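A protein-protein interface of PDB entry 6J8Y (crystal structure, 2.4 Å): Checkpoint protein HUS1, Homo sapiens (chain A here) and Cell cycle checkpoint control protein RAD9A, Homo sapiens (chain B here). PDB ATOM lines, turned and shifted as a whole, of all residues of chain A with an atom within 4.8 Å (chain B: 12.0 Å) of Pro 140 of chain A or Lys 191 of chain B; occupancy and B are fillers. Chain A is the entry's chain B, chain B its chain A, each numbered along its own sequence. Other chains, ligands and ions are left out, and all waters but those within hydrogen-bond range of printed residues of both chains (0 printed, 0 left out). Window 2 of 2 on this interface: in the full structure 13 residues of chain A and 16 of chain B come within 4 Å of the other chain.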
ATOM      1  N   GLU A  88     -19.559  16.015  11.118  1.00  0.00           N
ATOM      2  CA  GLU A  88     -20.481  14.903  10.959  1.00  0.00           C
ATOM      3  C   GLU A  88     -21.560  14.983  12.031  1.00  0.00           C
ATOM      4  O   GLU A  88     -21.258  15.149  13.213  1.00  0.00           O
ATOM      5  CB  GLU A  88     -19.740  13.567  11.034  1.00  0.00           C
ATOM      6  CG  GLU A  88     -20.643  12.356  10.887  1.00  0.00           C
ATOM      7  CD  GLU A  88     -19.869  11.058  10.760  1.00  0.00           C
ATOM      8  OE1 GLU A  88     -18.956  10.988   9.911  1.00  0.00           O
ATOM      9  OE2 GLU A  88     -20.178  10.107  11.509  1.00  0.00           O
ATOM     10  N   LEU A  89     -22.817  14.879  11.615  1.00  0.00           N
ATOM     11  CA  LEU A  89     -23.931  14.927  12.555  1.00  0.00           C
ATOM     12  C   LEU A  89     -25.077  14.023  12.114  1.00  0.00           C
ATOM     13  O   LEU A  89     -25.093  13.529  10.985  1.00  0.00           O
ATOM     14  CB  LEU A  89     -24.425  16.370  12.729  1.00  0.00           C
ATOM     15  CG  LEU A  89     -24.674  17.246  11.494  1.00  0.00           C
ATOM     16  CD1 LEU A  89     -25.978  16.899  10.783  1.00  0.00           C
ATOM     17  CD2 LEU A  89     -24.657  18.717  11.882  1.00  0.00           C
ATOM     18  N   ASN A  93     -31.447  15.073  13.919  1.00  0.00           N
ATOM     19  CA  ASN A  93     -31.184  16.175  14.841  1.00  0.00           C
ATOM     20  C   ASN A  93     -31.304  17.539  14.174  1.00  0.00           C
ATOM     21  O   ASN A  93     -31.937  18.448  14.712  1.00  0.00           O
ATOM     22  CB  ASN A  93     -29.794  16.027  15.462  1.00  0.00           C
ATOM     23  CG  ASN A  93     -29.727  14.903  16.476  1.00  0.00           C
ATOM     24  OD1 ASN A  93     -30.618  14.057  16.541  1.00  0.00           O
ATOM     25  ND2 ASN A  93     -28.664  14.888  17.271  1.00  0.00           N
ATOM     26  N   PHE A 116     -19.510  19.537  25.018  1.00  0.00           N
ATOM     27  CA  PHE A 116     -18.836  18.847  23.923  1.00  0.00           C
ATOM     28  C   PHE A 116     -19.048  19.626  22.622  1.00  0.00           C
ATOM     29  O   PHE A 116     -19.961  20.450  22.546  1.00  0.00           O
ATOM     30  CB  PHE A 116     -19.347  17.405  23.794  1.00  0.00           C
ATOM     31  CG  PHE A 116     -20.846  17.282  23.742  1.00  0.00           C
ATOM     32  CD1 PHE A 116     -21.586  17.188  24.907  1.00  0.00           C
ATOM     33  CD2 PHE A 116     -21.511  17.235  22.529  1.00  0.00           C
ATOM     34  CE1 PHE A 116     -22.962  17.071  24.868  1.00  0.00           C
ATOM     35  CE2 PHE A 116     -22.888  17.111  22.484  1.00  0.00           C
ATOM     36  CZ  PHE A 116     -23.614  17.032  23.655  1.00  0.00           C
ATOM     37  N   PRO A 117     -18.196  19.389  21.604  1.00  0.00           N
ATOM     38  CA  PRO A 117     -18.349  20.073  20.312  1.00  0.00           C
ATOM     39  C   PRO A 117     -19.765  19.968  19.746  1.00  0.00           C
ATOM     40  O   PRO A 117     -20.287  18.868  19.555  1.00  0.00           O
ATOM     41  CB  PRO A 117     -17.337  19.354  19.404  1.00  0.00           C
ATOM     42  CG  PRO A 117     -16.887  18.138  20.173  1.00  0.00           C
ATOM     43  CD  PRO A 117     -17.007  18.520  21.608  1.00  0.00           C
ATOM     44  N   CYS A 118     -20.377  21.121  19.493  1.00  0.00           N
ATOM     45  CA  CYS A 118     -21.767  21.179  19.065  1.00  0.00           C
ATOM     46  C   CYS A 118     -21.992  22.176  17.939  1.00  0.00           C
ATOM     47  O   CYS A 118     -21.253  23.150  17.794  1.00  0.00           O
ATOM     48  CB  CYS A 118     -22.674  21.551  20.241  1.00  0.00           C
ATOM     49  SG  CYS A 118     -23.258  20.168  21.230  1.00  0.00           S
ATOM     50  N   ASP A 138     -28.665  22.106  20.684  1.00  0.00           N
ATOM     51  CA  ASP A 138     -27.239  21.822  20.603  1.00  0.00           C
ATOM     52  C   ASP A 138     -27.001  20.489  19.909  1.00  0.00           C
ATOM     53  O   ASP A 138     -27.043  19.432  20.537  1.00  0.00           O
ATOM     54  CB  ASP A 138     -26.609  21.824  21.995  1.00  0.00           C
ATOM     55  CG  ASP A 138     -26.729  23.171  22.683  1.00  0.00           C
ATOM     56  OD1 ASP A 138     -26.578  24.203  21.996  1.00  0.00           O
ATOM     57  OD2 ASP A 138     -26.979  23.200  23.907  1.00  0.00           O
ATOM     58  N   ILE A 139     -26.760  20.552  18.602  1.00  0.00           N
ATOM     59  CA  ILE A 139     -26.521  19.361  17.796  1.00  0.00           C
ATOM     60  C   ILE A 139     -25.102  18.841  17.979  1.00  0.00           C
ATOM     61  O   ILE A 139     -24.142  19.517  17.609  1.00  0.00           O
ATOM     62  CB  ILE A 139     -26.749  19.644  16.299  1.00  0.00           C
ATOM     63  CG1 ILE A 139     -28.105  20.314  16.077  1.00  0.00           C
ATOM     64  CG2 ILE A 139     -26.628  18.360  15.488  1.00  0.00           C
ATOM     65  CD1 ILE A 139     -28.388  20.637  14.630  1.00  0.00           C
ATOM     66  N   PRO A 140     -24.962  17.636  18.556  1.00  0.00           N
ATOM     67  CA  PRO A 140     -23.635  17.026  18.683  1.00  0.00           C
ATOM     68  C   PRO A 140     -23.007  16.818  17.313  1.00  0.00           C
ATOM     69  O   PRO A 140     -23.680  16.333  16.403  1.00  0.00           O
ATOM     70  CB  PRO A 140     -23.920  15.685  19.367  1.00  0.00           C
ATOM     71  CG  PRO A 140     -25.249  15.866  20.031  1.00  0.00           C
ATOM     72  CD  PRO A 140     -26.017  16.783  19.130  1.00  0.00           C
ATOM     73  N   ILE A 141     -21.743  17.195  17.160  1.00  0.00           N
ATOM     74  CA  ILE A 141     -21.065  17.028  15.884  1.00  0.00           C
ATOM     75  C   ILE A 141     -19.716  16.346  16.054  1.00  0.00           C
ATOM     76  O   ILE A 141     -19.063  16.478  17.088  1.00  0.00           O
ATOM     77  CB  ILE A 141     -20.862  18.378  15.165  1.00  0.00           C
ATOM     78  CG1 ILE A 141     -20.161  19.380  16.085  1.00  0.00           C
ATOM     79  CG2 ILE A 141     -22.193  18.937  14.689  1.00  0.00           C
ATOM     80  CD1 ILE A 141     -18.709  19.615  15.737  1.00  0.00           C
ATOM     81  N   LYS A 142     -19.316  15.605  15.028  1.00  0.00           N
ATOM     82  CA  LYS A 142     -18.006  14.977  14.990  1.00  0.00           C
ATOM     83  C   LYS A 142     -17.118  15.728  14.002  1.00  0.00           C
ATOM     84  O   LYS A 142     -17.458  15.855  12.825  1.00  0.00           O
ATOM     85  CB  LYS A 142     -18.129  13.502  14.600  1.00  0.00           C
ATOM     86  CG  LYS A 142     -16.823  12.726  14.635  1.00  0.00           C
ATOM     87  CD  LYS A 142     -17.032  11.294  14.162  1.00  0.00           C
ATOM     88  CE  LYS A 142     -15.735  10.503  14.191  1.00  0.00           C
ATOM     89  NZ  LYS A 142     -14.670  11.148  13.373  1.00  0.00           N
ATOM     90  N   LEU B 163     -39.613  12.304  23.890  1.00  0.00           N
ATOM     91  CA  LEU B 163     -38.827  12.773  25.028  1.00  0.00           C
ATOM     92  C   LEU B 163     -39.504  12.408  26.347  1.00  0.00           C
ATOM     93  O   LEU B 163     -40.659  12.763  26.581  1.00  0.00           O
ATOM     94  CB  LEU B 163     -38.610  14.284  24.945  1.00  0.00           C
ATOM     95  CG  LEU B 163     -37.883  14.931  26.124  1.00  0.00           C
ATOM     96  CD1 LEU B 163     -36.473  14.379  26.257  1.00  0.00           C
ATOM     97  CD2 LEU B 163     -37.854  16.438  25.964  1.00  0.00           C
ATOM     98  N   SER B 180     -34.718  19.801  27.801  1.00  0.00           N
ATOM     99  CA  SER B 180     -34.784  18.349  27.718  1.00  0.00           C
ATOM    100  C   SER B 180     -33.763  17.717  28.660  1.00  0.00           C
ATOM    101  O   SER B 180     -32.666  18.244  28.844  1.00  0.00           O
ATOM    102  CB  SER B 180     -34.544  17.877  26.282  1.00  0.00           C
ATOM    103  OG  SER B 180     -33.269  18.283  25.816  1.00  0.00           O
ATOM    104  N   TYR B 181     -34.134  16.593  29.262  1.00  0.00           N
ATOM    105  CA  TYR B 181     -33.245  15.877  30.169  1.00  0.00           C
ATOM    106  C   TYR B 181     -32.814  14.559  29.539  1.00  0.00           C
ATOM    107  O   TYR B 181     -33.579  13.943  28.795  1.00  0.00           O
ATOM    108  CB  TYR B 181     -33.931  15.636  31.516  1.00  0.00           C
ATOM    109  CG  TYR B 181     -33.125  14.796  32.480  1.00  0.00           C
ATOM    110  CD1 TYR B 181     -32.214  15.384  33.350  1.00  0.00           C
ATOM    111  CD2 TYR B 181     -33.278  13.416  32.526  1.00  0.00           C
ATOM    112  CE1 TYR B 181     -31.476  14.619  34.233  1.00  0.00           C
ATOM    113  CE2 TYR B 181     -32.543  12.644  33.403  1.00  0.00           C
ATOM    114  CZ  TYR B 181     -31.645  13.249  34.255  1.00  0.00           C
ATOM    115  OH  TYR B 181     -30.915  12.482  35.132  1.00  0.00           O
ATOM    116  N   HIS B 182     -31.591  14.126  29.833  1.00  0.00           N
ATOM    117  CA  HIS B 182     -31.053  12.915  29.219  1.00  0.00           C
ATOM    118  C   HIS B 182     -30.189  12.106  30.184  1.00  0.00           C
ATOM    119  O   HIS B 182     -29.331  12.654  30.876  1.00  0.00           O
ATOM    120  CB  HIS B 182     -30.245  13.277  27.970  1.00  0.00           C
ATOM    121  CG  HIS B 182     -30.996  14.129  26.995  1.00  0.00           C
ATOM    122  ND1 HIS B 182     -31.912  13.610  26.104  1.00  0.00           N
ATOM    123  CD2 HIS B 182     -30.982  15.466  26.783  1.00  0.00           C
ATOM    124  CE1 HIS B 182     -32.423  14.589  25.381  1.00  0.00           C
ATOM    125  NE2 HIS B 182     -31.875  15.727  25.772  1.00  0.00           N
ATOM    126  N   GLU B 183     -30.425  10.798  30.220  1.00  0.00           N
ATOM    127  CA  GLU B 183     -29.666   9.892  31.077  1.00  0.00           C
ATOM    128  C   GLU B 183     -28.330   9.505  30.450  1.00  0.00           C
ATOM    129  O   GLU B 183     -27.941  10.046  29.414  1.00  0.00           O
ATOM    130  CB  GLU B 183     -30.473   8.625  31.372  1.00  0.00           C
ATOM    131  CG  GLU B 183     -31.716   8.841  32.216  1.00  0.00           C
ATOM    132  CD  GLU B 183     -32.475   7.550  32.463  1.00  0.00           C
ATOM    133  OE1 GLU B 183     -32.888   6.904  31.477  1.00  0.00           O
ATOM    134  OE2 GLU B 183     -32.652   7.177  33.642  1.00  0.00           O
ATOM    135  N   GLU B 184     -27.647   8.558  31.092  1.00  0.00           N
ATOM    136  CA  GLU B 184     -26.373   8.017  30.616  1.00  0.00           C
ATOM    137  C   GLU B 184     -25.362   9.106  30.263  1.00  0.00           C
ATOM    138  O   GLU B 184     -24.572   9.526  31.106  1.00  0.00           O
ATOM    139  CB  GLU B 184     -26.600   7.106  29.406  1.00  0.00           C
ATOM    140  CG  GLU B 184     -25.334   6.786  28.626  1.00  0.00           C
ATOM    141  CD  GLU B 184     -25.436   5.487  27.851  1.00  0.00           C
ATOM    142  OE1 GLU B 184     -26.353   5.363  27.012  1.00  0.00           O
ATOM    143  OE2 GLU B 184     -24.598   4.590  28.080  1.00  0.00           O
ATOM    144  N   THR B 189     -22.939   4.792  23.928  1.00  0.00           N
ATOM    145  CA  THR B 189     -22.095   5.962  24.135  1.00  0.00           C
ATOM    146  C   THR B 189     -22.176   6.908  22.940  1.00  0.00           C
ATOM    147  O   THR B 189     -21.207   7.084  22.200  1.00  0.00           O
ATOM    148  CB  THR B 189     -20.625   5.563  24.375  1.00  0.00           C
ATOM    149  OG1 THR B 189     -20.573   4.360  25.153  1.00  0.00           O
ATOM    150  CG2 THR B 189     -19.879   6.674  25.106  1.00  0.00           C
ATOM    151  N   ALA B 190     -23.349   7.506  22.755  1.00  0.00           N
ATOM    152  CA  ALA B 190     -23.566   8.497  21.707  1.00  0.00           C
ATOM    153  C   ALA B 190     -24.450   9.612  22.250  1.00  0.00           C
ATOM    154  O   ALA B 190     -25.507   9.354  22.825  1.00  0.00           O
ATOM    155  CB  ALA B 190     -24.190   7.858  20.480  1.00  0.00           C
ATOM    156  N   LYS B 191     -24.017  10.852  22.056  1.00  0.00           N
ATOM    157  CA  LYS B 191     -24.597  11.990  22.759  1.00  0.00           C
ATOM    158  C   LYS B 191     -25.920  12.461  22.158  1.00  0.00           C
ATOM    159  O   LYS B 191     -26.151  12.347  20.953  1.00  0.00           O
ATOM    160  CB  LYS B 191     -23.584  13.133  22.785  1.00  0.00           C
ATOM    161  CG  LYS B 191     -22.173  12.665  22.450  1.00  0.00           C
ATOM    162  CD  LYS B 191     -21.103  13.533  23.078  1.00  0.00           C
ATOM    163  CE  LYS B 191     -20.947  13.194  24.551  1.00  0.00           C
ATOM    164  NZ  LYS B 191     -19.655  13.690  25.096  1.00  0.00           N
ATOM    165  N   ALA B 192     -26.789  12.991  23.015  1.00  0.00           N
ATOM    166  CA  ALA B 192     -28.116  13.423  22.598  1.00  0.00           C
ATOM    167  C   ALA B 192     -28.196  14.937  22.432  1.00  0.00           C
ATOM    168  O   ALA B 192     -27.597  15.692  23.199  1.00  0.00           O
ATOM    169  CB  ALA B 192     -29.159  12.949  23.598  1.00  0.00           C
ATOM    170  N   MET B 193     -28.937  15.372  21.419  1.00  0.00           N
ATOM    171  CA  MET B 193     -29.183  16.792  21.213  1.00  0.00           C
ATOM    172  C   MET B 193     -30.043  17.335  22.344  1.00  0.00           C
ATOM    173  O   MET B 193     -31.088  16.769  22.664  1.00  0.00           O
ATOM    174  CB  MET B 193     -29.866  17.037  19.864  1.00  0.00           C
ATOM    175  CG  MET B 193     -30.157  18.503  19.578  1.00  0.00           C
ATOM    176  SD  MET B 193     -30.889  18.778  17.953  1.00  0.00           S
ATOM    177  CE  MET B 193     -32.488  18.006  18.163  1.00  0.00           C
ATOM    178  N   VAL B 194     -29.601  18.427  22.958  1.00  0.00           N
ATOM    179  CA  VAL B 194     -30.390  19.051  24.010  1.00  0.00           C
ATOM    180  C   VAL B 194     -31.184  20.225  23.444  1.00  0.00           C
ATOM    181  O   VAL B 194     -30.668  21.041  22.677  1.00  0.00           O
ATOM    182  CB  VAL B 194     -29.509  19.514  25.196  1.00  0.00           C
ATOM    183  CG1 VAL B 194     -28.801  18.322  25.823  1.00  0.00           C
ATOM    184  CG2 VAL B 194     -28.495  20.549  24.756  1.00  0.00           C
ATOM    185  N   THR B 195     -32.461  20.280  23.802  1.00  0.00           N
ATOM    186  CA  THR B 195     -33.335  21.360  23.369  1.00  0.00           C
ATOM    187  C   THR B 195     -33.717  22.213  24.569  1.00  0.00           C
ATOM    188  O   THR B 195     -34.066  21.687  25.626  1.00  0.00           O
ATOM    189  CB  THR B 195     -34.605  20.822  22.680  1.00  0.00           C
ATOM    190  OG1 THR B 195     -34.240  20.095  21.500  1.00  0.00           O
ATOM    191  CG2 THR B 195     -35.543  21.962  22.299  1.00  0.00           C
ATOM    192  N   GLU B 196     -33.634  23.528  24.408  1.00  0.00           N
ATOM    193  CA  GLU B 196     -33.995  24.440  25.483  1.00  0.00           C
ATOM    194  C   GLU B 196     -34.902  25.562  24.996  1.00  0.00           C
ATOM    195  O   GLU B 196     -34.541  26.327  24.104  1.00  0.00           O
ATOM    196  CB  GLU B 196     -32.742  25.032  26.129  1.00  0.00           C
ATOM    197  CG  GLU B 196     -33.026  26.226  27.022  1.00  0.00           C
ATOM    198  CD  GLU B 196     -31.817  26.653  27.830  1.00  0.00           C
ATOM    199  OE1 GLU B 196     -31.042  25.769  28.252  1.00  0.00           O
ATOM    200  OE2 GLU B 196     -31.643  27.871  28.042  1.00  0.00           O
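The backbone carbonyl oxygen (O) of Asn 93 of chain A sits close to the side-chain sulfur (SD) of Met 193 of chain B, at 3.4 Å.
The backbone NH (N) of Asp 138 of chain A is in hydrogen-bond range of the backbone carbonyl oxygen (O) of Val 194 of chain B.
NE2 of His 182 of chain B is in hydrogen-bond range of O of Met 193 of chain B (3.4 Å).
The side-chain sulfur (SG) of Cys 118 of chain A sits close to the backbone carbonyl oxygen (O) of Ile 139 of chain A (3.8 Å).
The backbone carbonyl oxygen (O) of Phe 116 of chain A lies close to the side-chain sulfur (SG) of Cys 118 of chain A (3.6 Å).
Among the printed residues, merely in contact across the chains: Phe 116 of chain A with Lys 191 of chain B, Asp 138 of chain A with Met 193 of chain B, Ile 139 of chain A with Met 193 of chain B, Pro 140 of chain A with Lys 191 of chain B, Pro 140 of chain A with Ala 192 of chain B and Pro 140 of chain A with Met 193 of chain B.
Pro 140 of chain A touches just these residues of chain B: Lys 191, Ala 192 and Met 193.
Lys 191 of chain B touches just these residues of chain A: Phe 116 and Pro 140.
No residue of chain B comes within 4 Å of Leu 89 of chain A.
Asn 93 of chain A touches just one residue of chain B: Met 193 (3.4 Å).
Phe 116 of chain A touches just one residue of chain B: Lys 191 (3.8 Å).
No residue of chain B comes within 4 Å of Pro 117 of chain A.
Cys 118 of chain A touches none of the printed residues of chain B.
Of chain B, only Met 193 comes within 4 Å of Ile 139 of chain A.
Of the printed residues of chain A, Met 193 of chain B touches Asn 93 (3.4 Å), Asp 138 (3.4 Å), Ile 139 (3.7 Å) and Pro 140 (3.8 Å).
Printed residues of chain B within 4 Å of Asp 138 of chain A: Met 193 (3.4 Å) and Val 194 (3.0 Å).
Of the printed residues of chain A, Ala 192 of chain B touches Pro 140.
Of the printed residues of chain A, Val 194 of chain B touches Asp 138 (3.0 Å).
The nearest printed residue of chain B that does not touch Asp 138 of chain A is Ala 192 of chain B (4.6 Å).
Hydrophobic or aromatic side chains of chain B within 4 Å of the printed part of chain A: Met 193 and Val 194.
Along chain B the printed residues that touch a printed residue of chain A span positions 191 to 194.
Hydrophobic or aromatic side chains of chain A that line the printed part of chain B: Phe 116, Ile 139 and Pro 140.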
